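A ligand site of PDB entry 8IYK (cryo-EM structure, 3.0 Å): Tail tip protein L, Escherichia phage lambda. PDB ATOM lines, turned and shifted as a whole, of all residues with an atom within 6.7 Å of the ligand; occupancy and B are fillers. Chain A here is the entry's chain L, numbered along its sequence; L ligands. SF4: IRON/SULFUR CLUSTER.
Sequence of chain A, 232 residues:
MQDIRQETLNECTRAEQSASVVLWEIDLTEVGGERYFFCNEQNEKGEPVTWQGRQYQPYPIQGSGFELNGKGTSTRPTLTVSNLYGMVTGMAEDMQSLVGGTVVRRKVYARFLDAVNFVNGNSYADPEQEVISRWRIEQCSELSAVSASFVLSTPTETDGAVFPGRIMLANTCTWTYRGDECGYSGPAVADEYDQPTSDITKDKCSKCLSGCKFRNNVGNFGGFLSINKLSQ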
ATOM      1  N   THR A 172     -19.620   2.371 -27.900  1.00  0.00           N
ATOM      2  CA  THR A 172     -19.358   1.722 -26.625  1.00  0.00           C
ATOM      3  C   THR A 172     -18.938   2.775 -25.609  1.00  0.00           C
ATOM      4  O   THR A 172     -18.108   3.632 -25.916  1.00  0.00           O
ATOM      5  CB  THR A 172     -18.276   0.646 -26.759  1.00  0.00           C
ATOM      6  OG1 THR A 172     -18.763  -0.417 -27.584  1.00  0.00           O
ATOM      7  CG2 THR A 172     -17.912   0.066 -25.397  1.00  0.00           C
ATOM      8  N   CYS A 173     -19.498   2.697 -24.410  1.00  0.00           N
ATOM      9  CA  CYS A 173     -19.159   3.609 -23.322  1.00  0.00           C
ATOM     10  C   CYS A 173     -18.056   2.993 -22.470  1.00  0.00           C
ATOM     11  O   CYS A 173     -18.127   1.821 -22.087  1.00  0.00           O
ATOM     12  CB  CYS A 173     -20.380   3.917 -22.467  1.00  0.00           C
ATOM     13  SG  CYS A 173     -20.078   5.106 -21.135  1.00  0.00           S
ATOM     14  N   THR A 174     -17.035   3.789 -22.164  1.00  0.00           N
ATOM     15  CA  THR A 174     -15.925   3.350 -21.324  1.00  0.00           C
ATOM     16  C   THR A 174     -16.108   3.728 -19.857  1.00  0.00           C
ATOM     17  O   THR A 174     -15.245   3.403 -19.041  1.00  0.00           O
ATOM     18  CB  THR A 174     -14.605   3.929 -21.837  1.00  0.00           C
ATOM     19  OG1 THR A 174     -14.543   5.329 -21.531  1.00  0.00           O
ATOM     20  CG2 THR A 174     -14.497   3.746 -23.342  1.00  0.00           C
ATOM     21  N   TRP A 175     -17.199   4.413 -19.513  1.00  0.00           N
ATOM     22  CA  TRP A 175     -17.436   4.810 -18.135  1.00  0.00           C
ATOM     23  C   TRP A 175     -17.895   3.623 -17.302  1.00  0.00           C
ATOM     24  O   TRP A 175     -18.107   2.518 -17.809  1.00  0.00           O
ATOM     25  CB  TRP A 175     -18.465   5.939 -18.081  1.00  0.00           C
ATOM     26  CG  TRP A 175     -18.061   7.246 -18.708  1.00  0.00           C
ATOM     27  CD1 TRP A 175     -18.880   8.120 -19.375  1.00  0.00           C
ATOM     28  CD2 TRP A 175     -16.753   7.864 -18.715  1.00  0.00           C
ATOM     29  NE1 TRP A 175     -18.174   9.214 -19.804  1.00  0.00           N
ATOM     30  CE2 TRP A 175     -16.870   9.074 -19.406  1.00  0.00           C
ATOM     31  CE3 TRP A 175     -15.502   7.491 -18.201  1.00  0.00           C
ATOM     32  CZ2 TRP A 175     -15.784   9.924 -19.606  1.00  0.00           C
ATOM     33  CZ3 TRP A 175     -14.439   8.338 -18.405  1.00  0.00           C
ATOM     34  CH2 TRP A 175     -14.577   9.538 -19.096  1.00  0.00           C
ATOM     35  N   THR A 176     -18.051   3.853 -16.009  1.00  0.00           N
ATOM     36  CA  THR A 176     -18.589   2.856 -15.084  1.00  0.00           C
ATOM     37  C   THR A 176     -20.025   3.239 -14.741  1.00  0.00           C
ATOM     38  O   THR A 176     -20.275   4.377 -14.326  1.00  0.00           O
ATOM     39  CB  THR A 176     -17.742   2.775 -13.814  1.00  0.00           C
ATOM     40  OG1 THR A 176     -16.360   2.886 -14.143  1.00  0.00           O
ATOM     41  CG2 THR A 176     -17.979   1.443 -13.108  1.00  0.00           C
ATOM     42  N   TYR A 177     -20.946   2.301 -14.911  1.00  0.00           N
ATOM     43  CA  TYR A 177     -22.360   2.589 -14.717  1.00  0.00           C
ATOM     44  C   TYR A 177     -22.625   3.106 -13.310  1.00  0.00           C
ATOM     45  O   TYR A 177     -22.126   2.547 -12.330  1.00  0.00           O
ATOM     46  CB  TYR A 177     -23.201   1.344 -14.988  1.00  0.00           C
ATOM     47  CG  TYR A 177     -24.684   1.628 -15.044  1.00  0.00           C
ATOM     48  CD1 TYR A 177     -25.170   2.751 -15.695  1.00  0.00           C
ATOM     49  CD2 TYR A 177     -25.590   0.780 -14.433  1.00  0.00           C
ATOM     50  CE1 TYR A 177     -26.516   3.012 -15.744  1.00  0.00           C
ATOM     51  CE2 TYR A 177     -26.943   1.034 -14.484  1.00  0.00           C
ATOM     52  CZ  TYR A 177     -27.399   2.157 -15.137  1.00  0.00           C
ATOM     53  OH  TYR A 177     -28.745   2.417 -15.185  1.00  0.00           O
ATOM     54  N   ARG A 178     -23.405   4.173 -13.214  1.00  0.00           N
ATOM     55  CA  ARG A 178     -23.701   4.862 -11.968  1.00  0.00           C
ATOM     56  C   ARG A 178     -22.435   5.326 -11.250  1.00  0.00           C
ATOM     57  O   ARG A 178     -22.441   5.506 -10.026  1.00  0.00           O
ATOM     58  CB  ARG A 178     -24.548   3.997 -11.032  1.00  0.00           C
ATOM     59  CG  ARG A 178     -25.912   3.642 -11.592  1.00  0.00           C
ATOM     60  CD  ARG A 178     -26.811   3.031 -10.531  1.00  0.00           C
ATOM     61  NE  ARG A 178     -28.067   2.555 -11.103  1.00  0.00           N
ATOM     62  CZ  ARG A 178     -29.180   3.285 -11.167  1.00  0.00           C
ATOM     63  NH1 ARG A 178     -29.225   4.526 -10.718  1.00  0.00           N
ATOM     64  NH2 ARG A 178     -30.264   2.739 -11.704  1.00  0.00           N
ATOM     65  N   GLY A 179     -21.349   5.509 -11.990  1.00  0.00           N
ATOM     66  CA  GLY A 179     -20.098   5.981 -11.435  1.00  0.00           C
ATOM     67  C   GLY A 179     -19.996   7.485 -11.438  1.00  0.00           C
ATOM     68  O   GLY A 179     -20.997   8.207 -11.511  1.00  0.00           O
ATOM     69  N   GLU A 181     -18.022   9.590 -13.682  1.00  0.00           N
ATOM     70  CA  GLU A 181     -18.130  10.193 -15.011  1.00  0.00           C
ATOM     71  C   GLU A 181     -19.457   9.858 -15.677  1.00  0.00           C
ATOM     72  O   GLU A 181     -19.999  10.688 -16.416  1.00  0.00           O
ATOM     73  CB  GLU A 181     -16.967   9.759 -15.883  1.00  0.00           C
ATOM     74  CG  GLU A 181     -15.601   9.995 -15.260  1.00  0.00           C
ATOM     75  CD  GLU A 181     -15.143   8.850 -14.376  1.00  0.00           C
ATOM     76  OE1 GLU A 181     -15.791   7.781 -14.402  1.00  0.00           O
ATOM     77  OE2 GLU A 181     -14.136   9.028 -13.660  1.00  0.00           O
ATOM     78  N   CYS A 182     -19.986   8.653 -15.451  1.00  0.00           N
ATOM     79  CA  CYS A 182     -21.308   8.329 -15.973  1.00  0.00           C
ATOM     80  C   CYS A 182     -22.361   9.236 -15.361  1.00  0.00           C
ATOM     81  O   CYS A 182     -23.248   9.735 -16.071  1.00  0.00           O
ATOM     82  CB  CYS A 182     -21.643   6.859 -15.692  1.00  0.00           C
ATOM     83  SG  CYS A 182     -23.381   6.436 -15.891  1.00  0.00           S
ATOM     84  N   GLY A 183     -22.289   9.482 -14.057  1.00  0.00           N
ATOM     85  CA  GLY A 183     -23.146  10.453 -13.399  1.00  0.00           C
ATOM     86  C   GLY A 183     -24.628  10.162 -13.505  1.00  0.00           C
ATOM     87  O   GLY A 183     -25.433  11.090 -13.693  1.00  0.00           O
ATOM     88  N   TYR A 184     -25.020   8.896 -13.397  1.00  0.00           N
ATOM     89  CA  TYR A 184     -26.417   8.500 -13.457  1.00  0.00           C
ATOM     90  C   TYR A 184     -26.902   8.094 -12.078  1.00  0.00           C
ATOM     91  O   TYR A 184     -26.207   7.355 -11.362  1.00  0.00           O
ATOM     92  CB  TYR A 184     -26.626   7.357 -14.450  1.00  0.00           C
ATOM     93  CG  TYR A 184     -28.068   6.936 -14.554  1.00  0.00           C
ATOM     94  CD1 TYR A 184     -29.035   7.799 -15.046  1.00  0.00           C
ATOM     95  CD2 TYR A 184     -28.470   5.666 -14.162  1.00  0.00           C
ATOM     96  CE1 TYR A 184     -30.354   7.411 -15.140  1.00  0.00           C
ATOM     97  CE2 TYR A 184     -29.785   5.271 -14.249  1.00  0.00           C
ATOM     98  CZ  TYR A 184     -30.725   6.151 -14.740  1.00  0.00           C
ATOM     99  OH  TYR A 184     -32.037   5.759 -14.840  1.00  0.00           O
ATOM    100  N   CYS A 205     -26.235  -1.313 -17.544  1.00  0.00           N
ATOM    101  CA  CYS A 205     -26.190  -0.618 -18.822  1.00  0.00           C
ATOM    102  C   CYS A 205     -25.532  -1.490 -19.873  1.00  0.00           C
ATOM    103  O   CYS A 205     -24.495  -2.120 -19.612  1.00  0.00           O
ATOM    104  CB  CYS A 205     -25.453   0.707 -18.701  1.00  0.00           C
ATOM    105  SG  CYS A 205     -25.523   1.709 -20.187  1.00  0.00           S
ATOM    106  N   SER A 206     -26.122  -1.524 -21.065  1.00  0.00           N
ATOM    107  CA  SER A 206     -25.533  -2.253 -22.181  1.00  0.00           C
ATOM    108  C   SER A 206     -24.273  -1.594 -22.703  1.00  0.00           C
ATOM    109  O   SER A 206     -23.573  -2.199 -23.534  1.00  0.00           O
ATOM    110  CB  SER A 206     -26.554  -2.377 -23.315  1.00  0.00           C
ATOM    111  OG  SER A 206     -27.293  -1.185 -23.479  1.00  0.00           O
ATOM    112  N   LYS A 207     -23.975  -0.371 -22.264  1.00  0.00           N
ATOM    113  CA  LYS A 207     -22.843   0.448 -22.682  1.00  0.00           C
ATOM    114  C   LYS A 207     -22.929   0.878 -24.146  1.00  0.00           C
ATOM    115  O   LYS A 207     -21.995   1.502 -24.645  1.00  0.00           O
ATOM    116  CB  LYS A 207     -21.487  -0.244 -22.444  1.00  0.00           C
ATOM    117  CG  LYS A 207     -21.323  -0.775 -21.030  1.00  0.00           C
ATOM    118  CD  LYS A 207     -21.055   0.358 -20.049  1.00  0.00           C
ATOM    119  CE  LYS A 207     -20.547  -0.188 -18.732  1.00  0.00           C
ATOM    120  NZ  LYS A 207     -19.437   0.641 -18.188  1.00  0.00           N
ATOM    121  N   CYS A 208     -24.022   0.565 -24.828  1.00  0.00           N
ATOM    122  CA  CYS A 208     -24.252   1.048 -26.176  1.00  0.00           C
ATOM    123  C   CYS A 208     -25.030   2.367 -26.121  1.00  0.00           C
ATOM    124  O   CYS A 208     -25.385   2.861 -25.047  1.00  0.00           O
ATOM    125  CB  CYS A 208     -25.019  -0.004 -26.988  1.00  0.00           C
ATOM    126  SG  CYS A 208     -24.310  -1.652 -26.907  1.00  0.00           S
ATOM    127  N   LEU A 209     -25.281   2.946 -27.292  1.00  0.00           N
ATOM    128  CA  LEU A 209     -26.020   4.205 -27.330  1.00  0.00           C
ATOM    129  C   LEU A 209     -27.464   4.012 -26.869  1.00  0.00           C
ATOM    130  O   LEU A 209     -28.024   4.888 -26.210  1.00  0.00           O
ATOM    131  CB  LEU A 209     -25.975   4.813 -28.723  1.00  0.00           C
ATOM    132  CG  LEU A 209     -26.556   6.220 -28.823  1.00  0.00           C
ATOM    133  CD1 LEU A 209     -25.936   7.133 -27.783  1.00  0.00           C
ATOM    134  CD2 LEU A 209     -26.368   6.800 -30.216  1.00  0.00           C
ATOM    135  N   GLY A 211     -28.605   1.886 -24.649  1.00  0.00           N
ATOM    136  CA  GLY A 211     -28.617   1.827 -23.190  1.00  0.00           C
ATOM    137  C   GLY A 211     -28.532   3.203 -22.562  1.00  0.00           C
ATOM    138  O   GLY A 211     -29.168   3.470 -21.540  1.00  0.00           O
ATOM    139  N   CYS A 212     -27.728   4.089 -23.155  1.00  0.00           N
ATOM    140  CA  CYS A 212     -27.633   5.448 -22.654  1.00  0.00           C
ATOM    141  C   CYS A 212     -28.928   6.220 -22.877  1.00  0.00           C
ATOM    142  O   CYS A 212     -29.375   6.965 -22.003  1.00  0.00           O
ATOM    143  CB  CYS A 212     -26.457   6.176 -23.318  1.00  0.00           C
ATOM    144  SG  CYS A 212     -25.559   7.273 -22.220  1.00  0.00           S
ATOM    145  N   LYS A 213     -29.557   6.037 -24.042  1.00  0.00           N
ATOM    146  CA  LYS A 213     -30.828   6.704 -24.320  1.00  0.00           C
ATOM    147  C   LYS A 213     -31.922   6.220 -23.374  1.00  0.00           C
ATOM    148  O   LYS A 213     -32.812   6.995 -23.023  1.00  0.00           O
ATOM    149  CB  LYS A 213     -31.251   6.461 -25.775  1.00  0.00           C
ATOM    150  CG  LYS A 213     -30.267   6.987 -26.801  1.00  0.00           C
ATOM    151  CD  LYS A 213     -30.976   7.808 -27.862  1.00  0.00           C
ATOM    152  CE  LYS A 213     -30.292   7.674 -29.214  1.00  0.00           C
ATOM    153  NZ  LYS A 213     -30.707   6.430 -29.924  1.00  0.00           N
ATOM    154  N   ARG A 215     -31.643   5.794 -20.353  1.00  0.00           N
ATOM    155  CA  ARG A 215     -31.486   6.593 -19.156  1.00  0.00           C
ATOM    156  C   ARG A 215     -31.428   8.089 -19.428  1.00  0.00           C
ATOM    157  O   ARG A 215     -31.227   8.877 -18.490  1.00  0.00           O
ATOM    158  CB  ARG A 215     -30.230   6.161 -18.404  1.00  0.00           C
ATOM    159  CG  ARG A 215     -30.324   4.755 -17.832  1.00  0.00           C
ATOM    160  CD  ARG A 215     -29.191   3.875 -18.312  1.00  0.00           C
ATOM    161  NE  ARG A 215     -29.203   2.577 -17.665  1.00  0.00           N
ATOM    162  CZ  ARG A 215     -29.578   1.451 -18.254  1.00  0.00           C
ATOM    163  NH1 ARG A 215     -29.994   1.431 -19.511  1.00  0.00           N
ATOM    164  NH2 ARG A 215     -29.561   0.311 -17.559  1.00  0.00           N
ATOM    165  N   ASN A 217     -29.122   9.739 -20.783  1.00  0.00           N
ATOM    166  CA  ASN A 217     -27.792  10.143 -20.367  1.00  0.00           C
ATOM    167  C   ASN A 217     -26.840  10.331 -21.538  1.00  0.00           C
ATOM    168  O   ASN A 217     -25.621  10.251 -21.365  1.00  0.00           O
ATOM    169  CB  ASN A 217     -27.225   9.124 -19.376  1.00  0.00           C
ATOM    170  CG  ASN A 217     -26.581   9.768 -18.175  1.00  0.00           C
ATOM    171  OD1 ASN A 217     -27.179  10.627 -17.527  1.00  0.00           O
ATOM    172  ND2 ASN A 217     -25.370   9.349 -17.848  1.00  0.00           N
ATOM    173  N   VAL A 218     -27.375  10.570 -22.734  1.00  0.00           N
ATOM    174  CA  VAL A 218     -26.542  10.640 -23.939  1.00  0.00           C
ATOM    175  C   VAL A 218     -25.512  11.757 -23.820  1.00  0.00           C
ATOM    176  O   VAL A 218     -24.431  11.674 -24.411  1.00  0.00           O
ATOM    177  CB  VAL A 218     -27.420  10.819 -25.187  1.00  0.00           C
ATOM    178  CG1 VAL A 218     -26.595  10.714 -26.453  1.00  0.00           C
ATOM    179  CG2 VAL A 218     -28.534   9.786 -25.194  1.00  0.00           C
ATOM    180  N   ASN A 220     -23.740  12.368 -21.231  1.00  0.00           N
ATOM    181  CA  ASN A 220     -22.622  11.799 -20.491  1.00  0.00           C
ATOM    182  C   ASN A 220     -22.109  10.508 -21.108  1.00  0.00           C
ATOM    183  O   ASN A 220     -21.354   9.781 -20.459  1.00  0.00           O
ATOM    184  CB  ASN A 220     -23.026  11.562 -19.038  1.00  0.00           C
ATOM    185  CG  ASN A 220     -23.114  12.853 -18.248  1.00  0.00           C
ATOM    186  OD1 ASN A 220     -23.132  13.940 -18.814  1.00  0.00           O
ATOM    187  ND2 ASN A 220     -23.183  12.730 -16.925  1.00  0.00           N
ATOM    188  N   PHE A 221     -22.511  10.192 -22.331  1.00  0.00           N
ATOM    189  CA  PHE A 221     -22.024   8.996 -23.007  1.00  0.00           C
ATOM    190  C   PHE A 221     -20.501   9.043 -23.130  1.00  0.00           C
ATOM    191  O   PHE A 221     -19.938  10.065 -23.536  1.00  0.00           O
ATOM    192  CB  PHE A 221     -22.669   8.870 -24.377  1.00  0.00           C
ATOM    193  CG  PHE A 221     -22.403   7.564 -25.068  1.00  0.00           C
ATOM    194  CD1 PHE A 221     -22.584   6.368 -24.396  1.00  0.00           C
ATOM    195  CD2 PHE A 221     -21.980   7.529 -26.377  1.00  0.00           C
ATOM    196  CE1 PHE A 221     -22.331   5.167 -25.023  1.00  0.00           C
ATOM    197  CE2 PHE A 221     -21.727   6.329 -27.004  1.00  0.00           C
ATOM    198  CZ  PHE A 221     -21.911   5.149 -26.329  1.00  0.00           C
ATOM    199  N   GLY A 222     -19.856   7.943 -22.781  1.00  0.00           N
ATOM    200  CA  GLY A 222     -18.408   7.874 -22.797  1.00  0.00           C
ATOM    201  C   GLY A 222     -17.778   7.597 -24.138  1.00  0.00           C
ATOM    202  O   GLY A 222     -16.555   7.615 -24.246  1.00  0.00           O
ATOM    203  N   GLY A 223     -18.575   7.335 -25.170  1.00  0.00           N
ATOM    204  CA  GLY A 223     -18.077   7.116 -26.503  1.00  0.00           C
ATOM    205  C   GLY A 223     -18.054   8.388 -27.331  1.00  0.00           C
ATOM    206  O   GLY A 223     -18.451   9.460 -26.899  1.00  0.00           O
HETATM  207 FE1  SF4 L   1     -23.605   5.636 -17.993  1.00  0.00          FE
HETATM  208 FE2  SF4 L   1     -24.435   3.612 -19.637  1.00  0.00          FE
HETATM  209 FE3  SF4 L   1     -22.139   4.989 -20.206  1.00  0.00          FE
HETATM  210 FE4  SF4 L   1     -24.575   6.205 -20.486  1.00  0.00          FE
HETATM  211  S1  SF4 L   1     -23.799   4.418 -21.666  1.00  0.00           S
HETATM  212  S2  SF4 L   1     -22.710   7.077 -19.503  1.00  0.00           S
HETATM  213  S3  SF4 L   1     -25.727   5.272 -18.749  1.00  0.00           S
HETATM  214  S4  SF4 L   1     -22.528   3.665 -18.394  1.00  0.00           S
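An iron atom (FE4) of the ligand is bound by the side-chain sulfur (SG) of Cys 212.
The side-chain sulfur (SG) of Cys 182 binds an iron atom (FE1) of the ligand.
FE2 of the ligand is bound by SG of Cys 205 (2.3 Å).
FE3 of the ligand is bound by SG of Cys 173.
The backbone carbonyl oxygen (O) of Cys 182 sits at hydrogen-bond distance from the side-chain amide nitrogen (ND2) of Asn 220 (3.1 Å).
The side-chain sulfur (SG) of Cys 205 lies close to the backbone NH (N) of Lys 207, at 3.3 Å.
The guanidinium group (NE) of Arg 215 sits at hydrogen-bond distance from the side-chain hydroxyl (OH) of Tyr 177 (2.5 Å).
The side-chain sulfur (SG) of Cys 182 lies close to the backbone NH (N) of Arg 178 (3.5 Å).
SG of Cys 173 lies close to N of Trp 175 (3.4 Å).
N of Cys 173 is in hydrogen-bond range of O of Lys 207 (2.8 Å).
NH1 of Arg 215 lies within hydrogen-bond range of O of Gly 211 (3.0 Å).
SG of Cys 212 sits close to N of Val 218 (3.8 Å).
The backbone carbonyl oxygen (O) of Asn 220 lies close to a sulfur (S2) of the ligand, 3.2 Å away.
Trp 175 touches the ligand (CD1 to S2, 3.97 Å).
CA of Tyr 177 touches S4 of the ligand, 3.8 Å away.
CD of Lys 207 touches S4 of the ligand, 3.98 Å away.
Arg 215 touches the ligand (CD to S3, 3.8 Å).
Asn 217 touches the ligand (ND2 to S2, 3.9 Å).
Phe 221 touches the ligand.
Hydrophobic or aromatic side chains within 4 Å of the ligand: Trp 175, Tyr 177 and Phe 221.
Within 4 Å of the ligand: Cys 173, Trp 175, Tyr 177, Cys 182, Cys 205, Lys 207, Cys 212, Arg 215, Asn 217, Asn 220 and Phe 221.
Along chain A the residues within 4 Å of the ligand span positions 173 to 221.
The nearest printed residue that does not touch the ligand is Cys 208 (4.05 Å).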
